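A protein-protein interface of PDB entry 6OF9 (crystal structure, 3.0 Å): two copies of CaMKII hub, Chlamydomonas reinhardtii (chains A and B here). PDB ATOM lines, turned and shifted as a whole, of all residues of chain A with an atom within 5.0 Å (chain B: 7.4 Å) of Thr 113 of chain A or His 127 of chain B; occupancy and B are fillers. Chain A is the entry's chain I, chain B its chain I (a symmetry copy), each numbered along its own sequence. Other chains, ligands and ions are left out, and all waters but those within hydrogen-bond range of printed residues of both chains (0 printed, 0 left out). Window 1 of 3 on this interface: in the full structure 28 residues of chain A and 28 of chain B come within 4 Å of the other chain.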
ATOM      1  N   ARG A  82      17.942  28.149  18.950  1.00  0.00           N
ATOM      2  CA  ARG A  82      17.393  26.800  18.998  1.00  0.00           C
ATOM      3  C   ARG A  82      17.646  26.215  20.378  1.00  0.00           C
ATOM      4  O   ARG A  82      18.794  26.162  20.830  1.00  0.00           O
ATOM      5  CB  ARG A  82      18.018  25.911  17.923  1.00  0.00           C
ATOM      6  CG  ARG A  82      17.767  24.427  18.133  1.00  0.00           C
ATOM      7  CD  ARG A  82      16.813  23.883  17.092  1.00  0.00           C
ATOM      8  NE  ARG A  82      17.296  24.153  15.742  1.00  0.00           N
ATOM      9  CZ  ARG A  82      16.643  23.823  14.634  1.00  0.00           C
ATOM     10  NH1 ARG A  82      15.473  23.204  14.709  1.00  0.00           N
ATOM     11  NH2 ARG A  82      17.161  24.111  13.450  1.00  0.00           N
ATOM     12  N   VAL A  90      21.541  27.063  20.816  1.00  0.00           N
ATOM     13  CA  VAL A  90      22.345  27.279  19.617  1.00  0.00           C
ATOM     14  C   VAL A  90      21.921  28.604  19.000  1.00  0.00           C
ATOM     15  O   VAL A  90      20.760  28.766  18.604  1.00  0.00           O
ATOM     16  CB  VAL A  90      22.181  26.130  18.612  1.00  0.00           C
ATOM     17  CG1 VAL A  90      23.086  26.348  17.407  1.00  0.00           C
ATOM     18  CG2 VAL A  90      22.472  24.795  19.277  1.00  0.00           C
ATOM     19  N   VAL A  91      22.856  29.549  18.915  1.00  0.00           N
ATOM     20  CA  VAL A  91      22.605  30.867  18.346  1.00  0.00           C
ATOM     21  C   VAL A  91      23.261  30.916  16.974  1.00  0.00           C
ATOM     22  O   VAL A  91      24.490  30.813  16.863  1.00  0.00           O
ATOM     23  CB  VAL A  91      23.142  31.985  19.253  1.00  0.00           C
ATOM     24  CG1 VAL A  91      22.817  33.349  18.668  1.00  0.00           C
ATOM     25  CG2 VAL A  91      22.566  31.852  20.647  1.00  0.00           C
ATOM     26  N   SER A  92      22.449  31.073  15.932  1.00  0.00           N
ATOM     27  CA  SER A  92      22.926  31.150  14.558  1.00  0.00           C
ATOM     28  C   SER A  92      22.534  32.502  13.980  1.00  0.00           C
ATOM     29  O   SER A  92      21.357  32.871  14.008  1.00  0.00           O
ATOM     30  CB  SER A  92      22.335  30.022  13.710  1.00  0.00           C
ATOM     31  OG  SER A  92      22.318  28.801  14.428  1.00  0.00           O
ATOM     32  N   GLU A 111      29.239  34.266   8.890  1.00  0.00           N
ATOM     33  CA  GLU A 111      28.263  33.325   9.425  1.00  0.00           C
ATOM     34  C   GLU A 111      28.754  32.823  10.777  1.00  0.00           C
ATOM     35  O   GLU A 111      29.888  32.347  10.887  1.00  0.00           O
ATOM     36  CB  GLU A 111      28.064  32.152   8.464  1.00  0.00           C
ATOM     37  CG  GLU A 111      27.659  32.551   7.052  1.00  0.00           C
ATOM     38  CD  GLU A 111      27.747  31.400   6.062  1.00  0.00           C
ATOM     39  OE1 GLU A 111      28.716  30.616   6.146  1.00  0.00           O
ATOM     40  OE2 GLU A 111      26.848  31.277   5.202  1.00  0.00           O
ATOM     41  N   GLU A 112      27.917  32.933  11.812  1.00  0.00           N
ATOM     42  CA  GLU A 112      28.341  32.541  13.151  1.00  0.00           C
ATOM     43  C   GLU A 112      27.321  31.616  13.792  1.00  0.00           C
ATOM     44  O   GLU A 112      26.125  31.931  13.846  1.00  0.00           O
ATOM     45  CB  GLU A 112      28.580  33.764  14.045  1.00  0.00           C
ATOM     46  CG  GLU A 112      29.914  34.452  13.788  1.00  0.00           C
ATOM     47  CD  GLU A 112      30.424  35.222  14.995  1.00  0.00           C
ATOM     48  OE1 GLU A 112      29.733  35.233  16.036  1.00  0.00           O
ATOM     49  OE2 GLU A 112      31.523  35.811  14.905  1.00  0.00           O
ATOM     50  N   THR A 113      27.809  30.469  14.270  1.00  0.00           N
ATOM     51  CA  THR A 113      27.061  29.549  15.117  1.00  0.00           C
ATOM     52  C   THR A 113      27.800  29.433  16.440  1.00  0.00           C
ATOM     53  O   THR A 113      28.964  29.019  16.468  1.00  0.00           O
ATOM     54  CB  THR A 113      26.927  28.167  14.471  1.00  0.00           C
ATOM     55  OG1 THR A 113      26.188  28.271  13.248  1.00  0.00           O
ATOM     56  CG2 THR A 113      26.214  27.213  15.413  1.00  0.00           C
ATOM     57  N   ARG A 114      27.132  29.799  17.529  1.00  0.00           N
ATOM     58  CA  ARG A 114      27.719  29.730  18.860  1.00  0.00           C
ATOM     59  C   ARG A 114      26.810  28.919  19.770  1.00  0.00           C
ATOM     60  O   ARG A 114      25.593  29.134  19.796  1.00  0.00           O
ATOM     61  CB  ARG A 114      27.959  31.131  19.436  1.00  0.00           C
ATOM     62  CG  ARG A 114      29.062  31.897  18.717  1.00  0.00           C
ATOM     63  CD  ARG A 114      29.366  33.223  19.394  1.00  0.00           C
ATOM     64  NE  ARG A 114      30.363  33.996  18.657  1.00  0.00           N
ATOM     65  CZ  ARG A 114      31.658  34.035  18.956  1.00  0.00           C
ATOM     66  NH1 ARG A 114      32.124  33.345  19.989  1.00  0.00           N
ATOM     67  NH2 ARG A 114      32.489  34.767  18.226  1.00  0.00           N
ATOM     68  N   VAL A 115      27.402  27.983  20.507  1.00  0.00           N
ATOM     69  CA  VAL A 115      26.665  27.076  21.377  1.00  0.00           C
ATOM     70  C   VAL A 115      26.893  27.496  22.821  1.00  0.00           C
ATOM     71  O   VAL A 115      28.038  27.718  23.242  1.00  0.00           O
ATOM     72  CB  VAL A 115      27.083  25.613  21.153  1.00  0.00           C
ATOM     73  CG1 VAL A 115      26.219  24.685  21.989  1.00  0.00           C
ATOM     74  CG2 VAL A 115      26.982  25.257  19.679  1.00  0.00           C
ATOM     75  N   HIS A 127      31.107  26.220  22.235  1.00  0.00           N
ATOM     76  CA  HIS A 127      31.510  25.960  20.860  1.00  0.00           C
ATOM     77  C   HIS A 127      31.248  27.184  19.994  1.00  0.00           C
ATOM     78  O   HIS A 127      30.275  27.916  20.199  1.00  0.00           O
ATOM     79  CB  HIS A 127      30.780  24.748  20.268  1.00  0.00           C
ATOM     80  CG  HIS A 127      31.198  24.423  18.867  1.00  0.00           C
ATOM     81  ND1 HIS A 127      32.495  24.099  18.537  1.00  0.00           N
ATOM     82  CD2 HIS A 127      30.493  24.385  17.712  1.00  0.00           C
ATOM     83  CE1 HIS A 127      32.572  23.869  17.238  1.00  0.00           C
ATOM     84  NE2 HIS A 127      31.371  24.037  16.714  1.00  0.00           N
ATOM     85  N   MET A 128      32.127  27.387  19.017  1.00  0.00           N
ATOM     86  CA  MET A 128      32.065  28.529  18.117  1.00  0.00           C
ATOM     87  C   MET A 128      32.414  28.079  16.708  1.00  0.00           C
ATOM     88  O   MET A 128      33.375  27.331  16.512  1.00  0.00           O
ATOM     89  CB  MET A 128      33.028  29.631  18.579  1.00  0.00           C
ATOM     90  CG  MET A 128      33.371  30.671  17.530  1.00  0.00           C
ATOM     91  SD  MET A 128      34.646  31.801  18.122  1.00  0.00           S
ATOM     92  CE  MET A 128      34.849  32.868  16.696  1.00  0.00           C
ATOM     93  N   HIS A 129      31.634  28.533  15.727  1.00  0.00           N
ATOM     94  CA  HIS A 129      31.892  28.221  14.322  1.00  0.00           C
ATOM     95  C   HIS A 129      31.658  29.485  13.506  1.00  0.00           C
ATOM     96  O   HIS A 129      30.518  29.942  13.372  1.00  0.00           O
ATOM     97  CB  HIS A 129      31.007  27.074  13.832  1.00  0.00           C
ATOM     98  CG  HIS A 129      31.387  26.552  12.481  1.00  0.00           C
ATOM     99  ND1 HIS A 129      32.309  27.177  11.670  1.00  0.00           N
ATOM    100  CD2 HIS A 129      30.968  25.460  11.797  1.00  0.00           C
ATOM    101  CE1 HIS A 129      32.440  26.497  10.545  1.00  0.00           C
ATOM    102  NE2 HIS A 129      31.636  25.451  10.596  1.00  0.00           N
ATOM    103  N   ASP B  31      15.655  17.021  11.374  1.00  0.00           N
ATOM    104  CA  ASP B  31      14.436  17.656  11.850  1.00  0.00           C
ATOM    105  C   ASP B  31      13.863  18.551  10.752  1.00  0.00           C
ATOM    106  O   ASP B  31      14.615  19.274  10.090  1.00  0.00           O
ATOM    107  CB  ASP B  31      14.722  18.472  13.114  1.00  0.00           C
ATOM    108  CG  ASP B  31      13.464  19.015  13.764  1.00  0.00           C
ATOM    109  OD1 ASP B  31      12.625  19.604  13.053  1.00  0.00           O
ATOM    110  OD2 ASP B  31      13.315  18.851  14.994  1.00  0.00           O
ATOM    111  N   SER B  33      12.608  21.277  10.847  1.00  0.00           N
ATOM    112  CA  SER B  33      12.939  22.670  11.124  1.00  0.00           C
ATOM    113  C   SER B  33      14.446  22.902  11.187  1.00  0.00           C
ATOM    114  O   SER B  33      14.908  23.791  11.911  1.00  0.00           O
ATOM    115  CB  SER B  33      12.279  23.119  12.426  1.00  0.00           C
ATOM    116  OG  SER B  33      12.787  22.389  13.530  1.00  0.00           O
ATOM    117  N   MET B  34      15.218  22.120  10.437  1.00  0.00           N
ATOM    118  CA  MET B  34      16.672  22.176  10.523  1.00  0.00           C
ATOM    119  C   MET B  34      17.213  23.484   9.954  1.00  0.00           C
ATOM    120  O   MET B  34      16.799  23.935   8.883  1.00  0.00           O
ATOM    121  CB  MET B  34      17.279  20.986   9.777  1.00  0.00           C
ATOM    122  CG  MET B  34      18.760  21.112   9.475  1.00  0.00           C
ATOM    123  SD  MET B  34      19.353  19.754   8.451  1.00  0.00           S
ATOM    124  CE  MET B  34      18.212  19.841   7.073  1.00  0.00           C
ATOM    125  N   THR B  35      18.149  24.089  10.683  1.00  0.00           N
ATOM    126  CA  THR B  35      18.830  25.301  10.251  1.00  0.00           C
ATOM    127  C   THR B  35      20.178  24.953   9.629  1.00  0.00           C
ATOM    128  O   THR B  35      20.818  23.964  10.000  1.00  0.00           O
ATOM    129  CB  THR B  35      19.028  26.271  11.420  1.00  0.00           C
ATOM    130  OG1 THR B  35      19.548  25.563  12.553  1.00  0.00           O
ATOM    131  CG2 THR B  35      17.710  26.930  11.793  1.00  0.00           C
ATOM    132  N   CYS B  36      20.614  25.785   8.684  1.00  0.00           N
ATOM    133  CA  CYS B  36      21.759  25.432   7.851  1.00  0.00           C
ATOM    134  C   CYS B  36      22.512  26.672   7.396  1.00  0.00           C
ATOM    135  O   CYS B  36      21.938  27.550   6.746  1.00  0.00           O
ATOM    136  CB  CYS B  36      21.302  24.619   6.638  1.00  0.00           C
ATOM    137  SG  CYS B  36      22.548  24.450   5.342  1.00  0.00           S
ATOM    138  N   PHE B  37      23.793  26.734   7.747  1.00  0.00           N
ATOM    139  CA  PHE B  37      24.783  27.548   7.055  1.00  0.00           C
ATOM    140  C   PHE B  37      25.579  26.629   6.140  1.00  0.00           C
ATOM    141  O   PHE B  37      26.081  25.596   6.589  1.00  0.00           O
ATOM    142  CB  PHE B  37      25.738  28.230   8.039  1.00  0.00           C
ATOM    143  CG  PHE B  37      25.183  29.461   8.693  1.00  0.00           C
ATOM    144  CD1 PHE B  37      24.493  30.410   7.959  1.00  0.00           C
ATOM    145  CD2 PHE B  37      25.375  29.677  10.048  1.00  0.00           C
ATOM    146  CE1 PHE B  37      23.998  31.547   8.569  1.00  0.00           C
ATOM    147  CE2 PHE B  37      24.880  30.808  10.663  1.00  0.00           C
ATOM    148  CZ  PHE B  37      24.188  31.743   9.925  1.00  0.00           C
ATOM    149  N   LEU B  45      21.272  32.171   6.424  1.00  0.00           N
ATOM    150  CA  LEU B  45      20.788  31.042   7.206  1.00  0.00           C
ATOM    151  C   LEU B  45      19.510  30.513   6.570  1.00  0.00           C
ATOM    152  O   LEU B  45      18.536  31.257   6.408  1.00  0.00           O
ATOM    153  CB  LEU B  45      20.542  31.452   8.657  1.00  0.00           C
ATOM    154  CG  LEU B  45      20.193  30.318   9.624  1.00  0.00           C
ATOM    155  CD1 LEU B  45      21.301  29.279   9.654  1.00  0.00           C
ATOM    156  CD2 LEU B  45      19.935  30.866  11.016  1.00  0.00           C
ATOM    157  N   VAL B  46      19.515  29.235   6.206  1.00  0.00           N
ATOM    158  CA  VAL B  46      18.388  28.594   5.542  1.00  0.00           C
ATOM    159  C   VAL B  46      17.745  27.609   6.506  1.00  0.00           C
ATOM    160  O   VAL B  46      18.433  26.964   7.307  1.00  0.00           O
ATOM    161  CB  VAL B  46      18.832  27.895   4.240  1.00  0.00           C
ATOM    162  CG1 VAL B  46      17.645  27.273   3.530  1.00  0.00           C
ATOM    163  CG2 VAL B  46      19.526  28.884   3.326  1.00  0.00           C
ATOM    164  N   ALA B  89      24.129  16.769  21.264  1.00  0.00           N
ATOM    165  CA  ALA B  89      25.499  16.419  20.910  1.00  0.00           C
ATOM    166  C   ALA B  89      25.962  17.283  19.746  1.00  0.00           C
ATOM    167  O   ALA B  89      25.269  17.394  18.731  1.00  0.00           O
ATOM    168  CB  ALA B  89      25.613  14.935  20.544  1.00  0.00           C
ATOM    169  N   VAL B  90      27.139  17.885  19.892  1.00  0.00           N
ATOM    170  CA  VAL B  90      27.729  18.742  18.869  1.00  0.00           C
ATOM    171  C   VAL B  90      28.917  18.006  18.266  1.00  0.00           C
ATOM    172  O   VAL B  90      29.882  17.693  18.975  1.00  0.00           O
ATOM    173  CB  VAL B  90      28.161  20.098  19.447  1.00  0.00           C
ATOM    174  CG1 VAL B  90      28.703  20.995  18.342  1.00  0.00           C
ATOM    175  CG2 VAL B  90      27.000  20.763  20.168  1.00  0.00           C
ATOM    176  N   VAL B  91      28.851  17.731  16.965  1.00  0.00           N
ATOM    177  CA  VAL B  91      29.911  17.036  16.245  1.00  0.00           C
ATOM    178  C   VAL B  91      30.648  18.061  15.395  1.00  0.00           C
ATOM    179  O   VAL B  91      30.060  18.658  14.483  1.00  0.00           O
ATOM    180  CB  VAL B  91      29.350  15.900  15.375  1.00  0.00           C
ATOM    181  CG1 VAL B  91      30.477  15.154  14.681  1.00  0.00           C
ATOM    182  CG2 VAL B  91      28.523  14.953  16.218  1.00  0.00           C
ATOM    183  N   THR B 113      30.216  21.679  11.533  1.00  0.00           N
ATOM    184  CA  THR B 113      29.607  21.553  12.850  1.00  0.00           C
ATOM    185  C   THR B 113      28.161  21.125  12.654  1.00  0.00           C
ATOM    186  O   THR B 113      27.385  21.837  12.008  1.00  0.00           O
ATOM    187  CB  THR B 113      29.660  22.873  13.626  1.00  0.00           C
ATOM    188  OG1 THR B 113      31.023  23.250  13.853  1.00  0.00           O
ATOM    189  CG2 THR B 113      28.946  22.728  14.960  1.00  0.00           C
ATOM    190  N   ARG B 114      27.803  19.969  13.202  1.00  0.00           N
ATOM    191  CA  ARG B 114      26.448  19.445  13.095  1.00  0.00           C
ATOM    192  C   ARG B 114      25.915  19.145  14.487  1.00  0.00           C
ATOM    193  O   ARG B 114      26.603  18.523  15.304  1.00  0.00           O
ATOM    194  CB  ARG B 114      26.402  18.194  12.210  1.00  0.00           C
ATOM    195  CG  ARG B 114      26.671  18.486  10.740  1.00  0.00           C
ATOM    196  CD  ARG B 114      26.487  17.251   9.873  1.00  0.00           C
ATOM    197  NE  ARG B 114      26.828  17.509   8.476  1.00  0.00           N
ATOM    198  CZ  ARG B 114      25.942  17.786   7.524  1.00  0.00           C
ATOM    199  NH1 ARG B 114      24.649  17.838   7.812  1.00  0.00           N
ATOM    200  NH2 ARG B 114      26.348  18.007   6.281  1.00  0.00           N
ATOM    201  N   VAL B 115      24.692  19.594  14.756  1.00  0.00           N
ATOM    202  CA  VAL B 115      24.064  19.450  16.063  1.00  0.00           C
ATOM    203  C   VAL B 115      22.990  18.378  15.970  1.00  0.00           C
ATOM    204  O   VAL B 115      22.156  18.397  15.051  1.00  0.00           O
ATOM    205  CB  VAL B 115      23.476  20.783  16.558  1.00  0.00           C
ATOM    206  CG1 VAL B 115      22.932  20.626  17.967  1.00  0.00           C
ATOM    207  CG2 VAL B 115      24.533  21.874  16.509  1.00  0.00           C
ATOM    208  N   TRP B 116      23.015  17.443  16.916  1.00  0.00           N
ATOM    209  CA  TRP B 116      22.062  16.349  16.986  1.00  0.00           C
ATOM    210  C   TRP B 116      21.335  16.409  18.321  1.00  0.00           C
ATOM    211  O   TRP B 116      21.931  16.738  19.352  1.00  0.00           O
ATOM    212  CB  TRP B 116      22.765  14.997  16.823  1.00  0.00           C
ATOM    213  CG  TRP B 116      23.487  14.852  15.516  1.00  0.00           C
ATOM    214  CD1 TRP B 116      24.711  15.365  15.192  1.00  0.00           C
ATOM    215  CD2 TRP B 116      23.030  14.143  14.358  1.00  0.00           C
ATOM    216  NE1 TRP B 116      25.041  15.021  13.903  1.00  0.00           N
ATOM    217  CE2 TRP B 116      24.027  14.271  13.369  1.00  0.00           C
ATOM    218  CE3 TRP B 116      21.876  13.414  14.060  1.00  0.00           C
ATOM    219  CZ2 TRP B 116      23.901  13.696  12.106  1.00  0.00           C
ATOM    220  CZ3 TRP B 116      21.754  12.844  12.807  1.00  0.00           C
ATOM    221  CH2 TRP B 116      22.760  12.987  11.845  1.00  0.00           C
ATOM    222  N   GLU B 117      20.042  16.096  18.290  1.00  0.00           N
ATOM    223  CA  GLU B 117      19.187  16.116  19.467  1.00  0.00           C
ATOM    224  C   GLU B 117      18.588  14.732  19.674  1.00  0.00           C
ATOM    225  O   GLU B 117      18.205  14.063  18.707  1.00  0.00           O
ATOM    226  CB  GLU B 117      18.069  17.158  19.315  1.00  0.00           C
ATOM    227  CG  GLU B 117      17.144  17.285  20.519  1.00  0.00           C
ATOM    228  CD  GLU B 117      16.028  18.289  20.293  1.00  0.00           C
ATOM    229  OE1 GLU B 117      15.748  18.616  19.121  1.00  0.00           O
ATOM    230  OE2 GLU B 117      15.435  18.756  21.288  1.00  0.00           O
ATOM    231  N   ILE B 124      18.424  12.995  16.006  1.00  0.00           N
ATOM    232  CA  ILE B 124      17.915  13.709  14.840  1.00  0.00           C
ATOM    233  C   ILE B 124      18.742  14.974  14.648  1.00  0.00           C
ATOM    234  O   ILE B 124      19.057  15.673  15.617  1.00  0.00           O
ATOM    235  CB  ILE B 124      16.416  14.044  14.990  1.00  0.00           C
ATOM    236  CG1 ILE B 124      15.590  12.761  15.099  1.00  0.00           C
ATOM    237  CG2 ILE B 124      15.927  14.868  13.815  1.00  0.00           C
ATOM    238  CD1 ILE B 124      15.564  11.946  13.822  1.00  0.00           C
ATOM    239  N   HIS B 125      19.094  15.259  13.397  1.00  0.00           N
ATOM    240  CA  HIS B 125      19.948  16.392  13.064  1.00  0.00           C
ATOM    241  C   HIS B 125      19.121  17.672  12.990  1.00  0.00           C
ATOM    242  O   HIS B 125      18.098  17.717  12.298  1.00  0.00           O
ATOM    243  CB  HIS B 125      20.649  16.123  11.733  1.00  0.00           C
ATOM    244  CG  HIS B 125      21.622  17.184  11.329  1.00  0.00           C
ATOM    245  ND1 HIS B 125      21.606  17.766  10.080  1.00  0.00           N
ATOM    246  CD2 HIS B 125      22.646  17.759  12.001  1.00  0.00           C
ATOM    247  CE1 HIS B 125      22.577  18.658  10.002  1.00  0.00           C
ATOM    248  NE2 HIS B 125      23.222  18.673  11.154  1.00  0.00           N
ATOM    249  N   VAL B 126      19.563  18.718  13.696  1.00  0.00           N
ATOM    250  CA  VAL B 126      18.754  19.931  13.803  1.00  0.00           C
ATOM    251  C   VAL B 126      19.464  21.147  13.215  1.00  0.00           C
ATOM    252  O   VAL B 126      18.816  22.034  12.645  1.00  0.00           O
ATOM    253  CB  VAL B 126      18.345  20.196  15.266  1.00  0.00           C
ATOM    254  CG1 VAL B 126      17.406  19.106  15.759  1.00  0.00           C
ATOM    255  CG2 VAL B 126      19.570  20.300  16.161  1.00  0.00           C
ATOM    256  N   HIS B 127      20.789  21.206  13.344  1.00  0.00           N
ATOM    257  CA  HIS B 127      21.544  22.358  12.872  1.00  0.00           C
ATOM    258  C   HIS B 127      22.803  21.901  12.148  1.00  0.00           C
ATOM    259  O   HIS B 127      23.420  20.896  12.510  1.00  0.00           O
ATOM    260  CB  HIS B 127      21.926  23.301  14.019  1.00  0.00           C
ATOM    261  CG  HIS B 127      22.669  24.521  13.568  1.00  0.00           C
ATOM    262  ND1 HIS B 127      22.133  25.432  12.684  1.00  0.00           N
ATOM    263  CD2 HIS B 127      23.910  24.973  13.868  1.00  0.00           C
ATOM    264  CE1 HIS B 127      23.009  26.396  12.463  1.00  0.00           C
ATOM    265  NE2 HIS B 127      24.096  26.140  13.169  1.00  0.00           N
ATOM    266  N   MET B 128      23.177  22.666  11.125  1.00  0.00           N
ATOM    267  CA  MET B 128      24.328  22.362  10.288  1.00  0.00           C
ATOM    268  C   MET B 128      25.067  23.650   9.962  1.00  0.00           C
ATOM    269  O   MET B 128      24.444  24.658   9.621  1.00  0.00           O
ATOM    270  CB  MET B 128      23.885  21.660   8.997  1.00  0.00           C
ATOM    271  CG  MET B 128      24.904  21.670   7.874  1.00  0.00           C
ATOM    272  SD  MET B 128      24.210  20.987   6.355  1.00  0.00           S
ATOM    273  CE  MET B 128      25.602  21.148   5.238  1.00  0.00           C
ATOM    274  N   HIS B 129      26.396  23.619  10.069  1.00  0.00           N
ATOM    275  CA  HIS B 129      27.229  24.771   9.732  1.00  0.00           C
ATOM    276  C   HIS B 129      28.450  24.268   8.974  1.00  0.00           C
ATOM    277  O   HIS B 129      29.313  23.597   9.552  1.00  0.00           O
ATOM    278  CB  HIS B 129      27.637  25.551  10.983  1.00  0.00           C
ATOM    279  CG  HIS B 129      28.288  26.868  10.690  1.00  0.00           C
ATOM    280  ND1 HIS B 129      28.669  27.247   9.422  1.00  0.00           N
ATOM    281  CD2 HIS B 129      28.625  27.896  11.505  1.00  0.00           C
ATOM    282  CE1 HIS B 129      29.216  28.449   9.467  1.00  0.00           C
ATOM    283  NE2 HIS B 129      29.202  28.865  10.719  1.00  0.00           N
ATOM    284  N   ARG B 130      28.530  24.610   7.691  1.00  0.00           N
ATOM    285  CA  ARG B 130      29.549  24.105   6.784  1.00  0.00           C
ATOM    286  C   ARG B 130      30.262  25.278   6.128  1.00  0.00           C
ATOM    287  O   ARG B 130      29.611  26.202   5.628  1.00  0.00           O
ATOM    288  CB  ARG B 130      28.912  23.196   5.725  1.00  0.00           C
ATOM    289  CG  ARG B 130      29.886  22.483   4.810  1.00  0.00           C
ATOM    290  CD  ARG B 130      29.164  21.421   3.989  1.00  0.00           C
ATOM    291  NE  ARG B 130      29.200  21.705   2.557  1.00  0.00           N
ATOM    292  CZ  ARG B 130      30.152  21.273   1.736  1.00  0.00           C
ATOM    293  NH1 ARG B 130      30.107  21.577   0.445  1.00  0.00           N
ATOM    294  NH2 ARG B 130      31.150  20.535   2.206  1.00  0.00           N
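Among the printed residues, pairs that only touch across the chains: His 129 of chain A with Thr 113 of chain B (3.0 Å), Thr 113 of chain A with His 129 of chain B (3.0 Å), Arg 82 of chain A with Met 34 of chain B (3.5 Å), Glu 111 of chain A with His 129 of chain B (3.6 Å), Thr 113 of chain A with Phe 37 of chain B (3.6 Å), Glu 112 of chain A with Phe 37 of chain B (3.6 Å), Ser 92 of chain A with Leu 45 of chain B (3.7 Å), Glu 111 of chain A with Phe 37 of chain B (3.7 Å), His 127 of chain A with Val 90 of chain B (3.9 Å) and Val 90 of chain A with His 127 of chain B (3.9 Å).
Of the 23 printed residues of chain B, 10 touch a printed residue of chain A. Hydrophobic or aromatic side chains of chain B that line the printed part of chain A: Phe 37, Leu 45, Val 90, His 127 and His 129. Of the 12 printed residues of chain A, 8 touch a printed residue of chain B. Among the printed residues, no Asp or Glu carboxylate lies within 4 Å of a Lys or Arg side-chain nitrogen of the other chain.
Of chain B, only Phe 37 (3.6 Å), His 127 (3.0 Å) and His 129 (3.0 Å) come within 4 Å of Thr 113 of chain A. Arg 114 of chain A touches none of the printed residues of chain B. Of the printed residues of chain B, His 129 of chain A touches Thr 113 (3.0 Å) and His 129 (3.2 Å). Printed residues of chain A within 4 Å of Phe 37 of chain B: Glu 111 (3.7 Å), Glu 112 (3.6 Å) and Thr 113 (3.6 Å). Val 91 of chain B touches none of the printed residues of chain A. His 127 of chain B touches three residues of chain A. The nearest residue of chain A that does not touch His 127 of chain B is Arg 82 of chain A (4.6 Å).
The backbone carbonyl oxygen (O) of Arg 82 of chain A is in hydrogen-bond range of the backbone NH (N) of Val 90 of chain A, at 2.9 Å. O of Thr 113 of chain A lies within hydrogen-bond range of N of His 129 of chain A, 2.8 Å away. The backbone NH of Val 115 of chain A lies within hydrogen-bond range of the backbone carbonyl oxygen of His 127 of chain A (2.9 Å). The side-chain hydroxyl (OG1) of Thr 35 of chain B lies within hydrogen-bond range of a ring nitrogen (ND1) of His 127 of chain B, 2.6 Å away. The backbone NH (N) of Met 128 of chain B sits at hydrogen-bond distance from the backbone carbonyl oxygen (O) of Thr 35 of chain B (2.9 Å). The backbone NH of Phe 37 of chain B lies within hydrogen-bond range of the backbone carbonyl oxygen of Met 128 of chain B.
Val 90 of chain A touches His 127 of chain B, and with the chains exchanged His 127 of chain A touches Val 90 of chain B. Thr 113 of chain A touches His 127 of chain B, and with the chains exchanged His 127 of chain A touches Thr 113 of chain B. Thr 113 of chain A touches His 129 of chain B, and with the chains exchanged His 129 of chain A touches Thr 113 of chain B. His 129 of chain B touches its own counterpart, His 129 of chain A. Positions printed for both chains: 90, 91, 113, 114, 115, 127, 128 and 129.
The backbone carbonyl oxygen (O) of Ser 33 of chain B lies within hydrogen-bond range of the guanidinium group (NH2) of Arg 82 of chain A (2.7 Å). NH2 of Arg 82 of chain A lies within hydrogen-bond range of OG1 of Thr 35 of chain B, at 2.9 Å. The guanidinium group of Arg 82 of chain A is in hydrogen-bond range of the backbone carbonyl oxygen of Val 126 of chain B (2.8 Å). The side-chain hydroxyl (OG) of Ser 92 of chain A lies close to a ring nitrogen (NE2) of His 127 of chain B (3.4 Å). A ring nitrogen (NE2) of His 127 of chain B lies within hydrogen-bond range of the side-chain hydroxyl (OG1) of Thr 113 of chain A (3.0 Å). A ring nitrogen (NE2) of His 127 of chain A sits at hydrogen-bond distance from the side-chain hydroxyl (OG1) of Thr 113 of chain B (3.0 Å). A ring nitrogen (NE2) of His 129 of chain B sits at hydrogen-bond distance from the backbone carbonyl oxygen of His 129 of chain A, at 3.2 Å.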
